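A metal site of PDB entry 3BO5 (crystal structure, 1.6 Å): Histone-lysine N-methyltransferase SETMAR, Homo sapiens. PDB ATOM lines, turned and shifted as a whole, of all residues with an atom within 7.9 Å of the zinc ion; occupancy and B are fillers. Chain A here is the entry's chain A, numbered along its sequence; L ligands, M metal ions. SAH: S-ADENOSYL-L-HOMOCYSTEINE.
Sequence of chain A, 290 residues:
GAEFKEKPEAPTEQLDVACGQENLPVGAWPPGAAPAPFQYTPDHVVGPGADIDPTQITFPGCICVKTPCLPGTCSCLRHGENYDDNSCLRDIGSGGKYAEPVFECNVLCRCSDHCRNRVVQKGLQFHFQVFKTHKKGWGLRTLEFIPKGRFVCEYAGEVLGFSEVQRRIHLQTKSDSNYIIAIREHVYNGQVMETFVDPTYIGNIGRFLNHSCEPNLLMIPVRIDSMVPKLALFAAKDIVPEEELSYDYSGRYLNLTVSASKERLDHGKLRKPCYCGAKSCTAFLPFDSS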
ATOM      1  N   HIS A 211      13.886  17.921  21.210  1.00  0.00           N
ATOM      2  CA  HIS A 211      13.692  17.317  22.493  1.00  0.00           C
ATOM      3  C   HIS A 211      14.669  16.157  22.694  1.00  0.00           C
ATOM      4  O   HIS A 211      15.013  15.435  21.803  1.00  0.00           O
ATOM      5  CB  HIS A 211      12.312  16.610  22.432  1.00  0.00           C
ATOM      6  CG  HIS A 211      12.072  15.700  23.571  1.00  0.00           C
ATOM      7  ND1 HIS A 211      11.810  16.168  24.851  1.00  0.00           N
ATOM      8  CD2 HIS A 211      12.096  14.341  23.647  1.00  0.00           C
ATOM      9  CE1 HIS A 211      11.684  15.126  25.664  1.00  0.00           C
ATOM     10  NE2 HIS A 211      11.885  14.011  24.961  1.00  0.00           N
ATOM     11  N   SER A 212      15.067  15.970  23.925  1.00  0.00           N
ATOM     12  CA  SER A 212      15.707  14.747  24.286  1.00  0.00           C
ATOM     13  C   SER A 212      15.164  14.269  25.598  1.00  0.00           C
ATOM     14  O   SER A 212      14.902  15.083  26.455  1.00  0.00           O
ATOM     15  CB  SER A 212      17.195  14.994  24.423  1.00  0.00           C
ATOM     16  OG  SER A 212      17.789  13.738  24.906  1.00  0.00           O
ATOM     17  N   CYS A 213      15.069  12.922  25.762  1.00  0.00           N
ATOM     18  CA  CYS A 213      14.681  12.347  27.026  1.00  0.00           C
ATOM     19  C   CYS A 213      15.796  12.471  28.064  1.00  0.00           C
ATOM     20  O   CYS A 213      15.566  12.269  29.254  1.00  0.00           O
ATOM     21  CB  CYS A 213      14.352  10.857  26.718  1.00  0.00           C
ATOM     22  SG  CYS A 213      12.825  10.760  25.770  1.00  0.00           S
ATOM     23  N   GLU A 214      17.010  12.730  27.569  1.00  0.00           N
ATOM     24  CA  GLU A 214      18.172  12.952  28.425  1.00  0.00           C
ATOM     25  C   GLU A 214      18.867  14.143  27.846  1.00  0.00           C
ATOM     26  O   GLU A 214      19.930  14.054  27.242  1.00  0.00           O
ATOM     27  CB  GLU A 214      19.119  11.743  28.420  1.00  0.00           C
ATOM     28  CG  GLU A 214      18.600  10.564  29.166  1.00  0.00           C
ATOM     29  CD  GLU A 214      19.558   9.370  29.092  1.00  0.00           C
ATOM     30  OE1 GLU A 214      20.765   9.541  28.745  1.00  0.00           O
ATOM     31  OE2 GLU A 214      19.054   8.254  29.376  1.00  0.00           O
ATOM     32  N   PRO A 273       6.611   9.902  17.693  1.00  0.00           N
ATOM     33  CA  PRO A 273       7.780   9.105  18.146  1.00  0.00           C
ATOM     34  C   PRO A 273       8.935  10.022  18.442  1.00  0.00           C
ATOM     35  O   PRO A 273       9.083  11.047  17.770  1.00  0.00           O
ATOM     36  CB  PRO A 273       8.170   8.279  16.948  1.00  0.00           C
ATOM     37  CG  PRO A 273       7.097   8.463  15.971  1.00  0.00           C
ATOM     38  CD  PRO A 273       6.310   9.675  16.264  1.00  0.00           C
ATOM     39  N   CYS A 274       9.721   9.612  19.422  1.00  0.00           N
ATOM     40  CA  CYS A 274      10.947  10.329  19.800  1.00  0.00           C
ATOM     41  C   CYS A 274      12.107   9.523  19.219  1.00  0.00           C
ATOM     42  O   CYS A 274      12.216   8.309  19.413  1.00  0.00           O
ATOM     43  CB  CYS A 274      11.082  10.388  21.359  1.00  0.00           C
ATOM     44  SG  CYS A 274      12.550  11.319  21.759  1.00  0.00           S
ATOM     45  N   TYR A 275      13.066  10.256  18.648  1.00  0.00           N
ATOM     46  CA  TYR A 275      14.284   9.684  18.067  1.00  0.00           C
ATOM     47  C   TYR A 275      15.523  10.270  18.791  1.00  0.00           C
ATOM     48  O   TYR A 275      16.606  10.422  18.168  1.00  0.00           O
ATOM     49  CB  TYR A 275      14.384   9.952  16.553  1.00  0.00           C
ATOM     50  CG  TYR A 275      13.159   9.544  15.786  1.00  0.00           C
ATOM     51  CD1 TYR A 275      12.676   8.227  15.948  1.00  0.00           C
ATOM     52  CD2 TYR A 275      12.549  10.403  14.908  1.00  0.00           C
ATOM     53  CE1 TYR A 275      11.555   7.798  15.215  1.00  0.00           C
ATOM     54  CE2 TYR A 275      11.399   9.993  14.182  1.00  0.00           C
ATOM     55  CZ  TYR A 275      10.940   8.678  14.357  1.00  0.00           C
ATOM     56  OH  TYR A 275       9.844   8.210  13.631  1.00  0.00           O
ATOM     57  N   CYS A 276      15.365  10.632  20.060  1.00  0.00           N
ATOM     58  CA  CYS A 276      16.441  11.336  20.737  1.00  0.00           C
ATOM     59  C   CYS A 276      17.636  10.436  20.920  1.00  0.00           C
ATOM     60  O   CYS A 276      18.717  10.973  21.045  1.00  0.00           O
ATOM     61  CB  CYS A 276      15.975  11.929  22.076  1.00  0.00           C
ATOM     62  SG  CYS A 276      15.832  10.742  23.444  1.00  0.00           S
ATOM     63  N   GLY A 277      17.455   9.103  20.940  1.00  0.00           N
ATOM     64  CA  GLY A 277      18.668   8.180  21.078  1.00  0.00           C
ATOM     65  C   GLY A 277      19.156   7.941  22.465  1.00  0.00           C
ATOM     66  O   GLY A 277      20.124   7.185  22.702  1.00  0.00           O
ATOM     67  N   ALA A 278      18.527   8.575  23.440  1.00  0.00           N
ATOM     68  CA  ALA A 278      18.921   8.362  24.833  1.00  0.00           C
ATOM     69  C   ALA A 278      18.582   6.950  25.327  1.00  0.00           C
ATOM     70  O   ALA A 278      17.540   6.373  24.943  1.00  0.00           O
ATOM     71  CB  ALA A 278      18.260   9.441  25.741  1.00  0.00           C
ATOM     72  N   LYS A 279      19.425   6.384  26.201  1.00  0.00           N
ATOM     73  CA  LYS A 279      19.090   5.081  26.789  1.00  0.00           C
ATOM     74  C   LYS A 279      17.732   5.054  27.513  1.00  0.00           C
ATOM     75  O   LYS A 279      17.026   4.049  27.448  1.00  0.00           O
ATOM     76  CB  LYS A 279      20.253   4.613  27.693  1.00  0.00           C
ATOM     77  CG  LYS A 279      21.563   4.551  26.908  1.00  0.00           C
ATOM     78  CD  LYS A 279      21.815   3.240  26.114  1.00  0.00           C
ATOM     79  CE  LYS A 279      22.153   3.438  24.588  1.00  0.00           C
ATOM     80  NZ  LYS A 279      23.413   4.116  24.142  1.00  0.00           N
ATOM     81  N   SER A 280      17.387   6.133  28.222  1.00  0.00           N
ATOM     82  CA  SER A 280      16.097   6.166  28.899  1.00  0.00           C
ATOM     83  C   SER A 280      14.983   6.686  27.985  1.00  0.00           C
ATOM     84  O   SER A 280      13.926   7.068  28.495  1.00  0.00           O
ATOM     85  CB  SER A 280      16.167   7.021  30.166  1.00  0.00           C
ATOM     86  OG  SER A 280      16.417   8.384  29.860  1.00  0.00           O
ATOM     87  N   CYS A 281      15.211   6.705  26.667  1.00  0.00           N
ATOM     88  CA  CYS A 281      14.120   7.197  25.760  1.00  0.00           C
ATOM     89  C   CYS A 281      12.781   6.541  26.049  1.00  0.00           C
ATOM     90  O   CYS A 281      12.718   5.313  26.295  1.00  0.00           O
ATOM     91  CB  CYS A 281      14.468   7.040  24.308  1.00  0.00           C
ATOM     92  SG  CYS A 281      13.305   7.898  23.155  1.00  0.00           S
ATOM     93  N   THR A 282      11.703   7.334  26.072  1.00  0.00           N
ATOM     94  CA  THR A 282      10.375   6.787  26.336  1.00  0.00           C
ATOM     95  C   THR A 282       9.706   6.391  25.025  1.00  0.00           C
ATOM     96  O   THR A 282       8.586   5.814  25.041  1.00  0.00           O
ATOM     97  CB  THR A 282       9.516   7.871  26.936  1.00  0.00           C
ATOM     98  OG1 THR A 282       9.435   8.952  25.992  1.00  0.00           O
ATOM     99  CG2 THR A 282      10.115   8.353  28.229  1.00  0.00           C
ATOM    100  N   ALA A 283      10.357   6.708  23.885  1.00  0.00           N
ATOM    101  CA  ALA A 283       9.896   6.488  22.514  1.00  0.00           C
ATOM    102  C   ALA A 283       8.805   7.460  22.062  1.00  0.00           C
ATOM    103  O   ALA A 283       8.362   7.389  20.901  1.00  0.00           O
ATOM    104  CB  ALA A 283       9.397   4.978  22.301  1.00  0.00           C
ATOM    105  N   PHE A 284       8.369   8.377  22.940  1.00  0.00           N
ATOM    106  CA  PHE A 284       7.421   9.376  22.474  1.00  0.00           C
ATOM    107  C   PHE A 284       7.828  10.775  22.862  1.00  0.00           C
ATOM    108  O   PHE A 284       8.390  11.027  23.948  1.00  0.00           O
ATOM    109  CB  PHE A 284       5.920   9.059  22.704  1.00  0.00           C
ATOM    110  CG  PHE A 284       5.144  10.075  23.642  1.00  0.00           C
ATOM    111  CD1 PHE A 284       5.418  10.202  24.974  1.00  0.00           C
ATOM    112  CD2 PHE A 284       4.086  10.833  23.139  1.00  0.00           C
ATOM    113  CE1 PHE A 284       4.716  11.091  25.798  1.00  0.00           C
ATOM    114  CE2 PHE A 284       3.376  11.751  23.942  1.00  0.00           C
ATOM    115  CZ  PHE A 284       3.673  11.859  25.279  1.00  0.00           C
ATOM    116  N   LEU A 285       7.503  11.698  21.965  1.00  0.00           N
ATOM    117  CA  LEU A 285       7.770  13.077  22.198  1.00  0.00           C
ATOM    118  C   LEU A 285       6.694  13.596  23.139  1.00  0.00           C
ATOM    119  O   LEU A 285       5.483  13.547  22.794  1.00  0.00           O
ATOM    120  CB  LEU A 285       7.772  13.773  20.806  1.00  0.00           C
ATOM    121  CG  LEU A 285       8.794  14.714  20.290  1.00  0.00           C
ATOM    122  CD1 LEU A 285      10.174  14.105  20.587  1.00  0.00           C
ATOM    123  CD2 LEU A 285       8.476  14.886  18.836  1.00  0.00           C
ATOM    124  N   PRO A 286       7.091  14.058  24.317  1.00  0.00           N
ATOM    125  CA  PRO A 286       6.109  14.351  25.379  1.00  0.00           C
ATOM    126  C   PRO A 286       5.441  15.736  25.283  1.00  0.00           C
ATOM    127  O   PRO A 286       5.545  16.527  26.242  1.00  0.00           O
ATOM    128  CB  PRO A 286       6.913  14.197  26.642  1.00  0.00           C
ATOM    129  CG  PRO A 286       8.346  14.774  26.207  1.00  0.00           C
ATOM    130  CD  PRO A 286       8.490  14.268  24.778  1.00  0.00           C
HETATM  131  N   SAH L   1      13.101  19.951  14.247  1.00  0.00           N
HETATM  132  CA  SAH L   1      12.443  21.291  14.320  1.00  0.00           C
HETATM  133  CB  SAH L   1      12.974  22.151  15.491  1.00  0.00           C
HETATM  134  CG  SAH L   1      12.294  21.696  16.800  1.00  0.00           C
HETATM  135  SD  SAH L   1      10.524  22.102  16.818  1.00  0.00           S
HETATM  136  C   SAH L   1      12.630  21.998  12.956  1.00  0.00           C
HETATM  137  O   SAH L   1      13.074  21.385  11.993  1.00  0.00           O
HETATM  138  OXT SAH L   1      12.298  23.232  12.890  1.00  0.00           O
HETATM  139  C5' SAH L   1       9.852  20.504  17.337  1.00  0.00           C
HETATM  140  C4' SAH L   1       9.746  19.469  16.213  1.00  0.00           C
HETATM  141  O4' SAH L   1      11.023  18.886  15.931  1.00  0.00           O
HETATM  142  C3' SAH L   1       8.882  18.291  16.580  1.00  0.00           C
HETATM  143  O3' SAH L   1       7.481  18.581  16.321  1.00  0.00           O
HETATM  144  C2' SAH L   1       9.398  17.188  15.708  1.00  0.00           C
HETATM  145  O2' SAH L   1       9.058  17.384  14.322  1.00  0.00           O
HETATM  146  C1' SAH L   1      10.896  17.459  15.777  1.00  0.00           C
HETATM  147  N9  SAH L   1      11.538  16.858  16.955  1.00  0.00           N
HETATM  148  C8  SAH L   1      12.150  17.513  18.028  1.00  0.00           C
HETATM  149  N7  SAH L   1      12.676  16.613  18.831  1.00  0.00           N
HETATM  150  C5  SAH L   1      12.472  15.382  18.302  1.00  0.00           C
HETATM  151  C6  SAH L   1      12.808  14.104  18.791  1.00  0.00           C
HETATM  152  N6  SAH L   1      13.530  13.841  19.880  1.00  0.00           N
HETATM  153  N1  SAH L   1      12.374  13.050  17.999  1.00  0.00           N
HETATM  154  C2  SAH L   1      11.667  13.248  16.848  1.00  0.00           C
HETATM  155  N3  SAH L   1      11.341  14.483  16.319  1.00  0.00           N
HETATM  156  C4  SAH L   1      11.721  15.506  17.141  1.00  0.00           C
HETATM  157 ZN    ZN M   1      13.620  10.148  23.548  1.00  0.00          ZN
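SG of Cys 274 sits close to N6 of the ligand, 3.3 Å away.
N7 of the ligand sits at hydrogen-bond distance from N of His 211, at 3.0 Å.
The backbone carbonyl oxygen of His 211 lies within hydrogen-bond range of a nitrogen (N6) of the ligand, at 2.9 Å.
The backbone NH of Tyr 275 sits at hydrogen-bond distance from a nitrogen (N1) of the ligand (3.0 Å).
SG of Cys 276 sits close to N of Ala 278, 3.5 Å away.
The side-chain sulfur (SG) of Cys 281 sits close to the backbone NH (N) of Ala 283 (3.3 Å).
N of Cys 274 is in hydrogen-bond range of O of Ala 283 (3.0 Å).
The backbone NH of Thr 282 sits close to the side-chain sulfur of Cys 213 (3.6 Å).
NE2 of His 211 lies within hydrogen-bond range of N of Cys 213 (3.5 Å).
Along chain A the residues within 4 Å of the zinc ion span positions 213 to 281.
The nearest printed residue that does not touch the zinc ion is Thr 282 (4.2 Å).
SG of Cys 276 is bound to the zinc ion, at 2.3 Å.
The zinc ion is bound by SG of Cys 281 (2.3 Å).
The side-chain sulfur (SG) of Cys 274 binds the zinc ion, 2.4 Å away.
SG of Cys 213 is bound to the zinc ion, at 2.4 Å.
The zinc ion has four donor atoms within binding distance.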
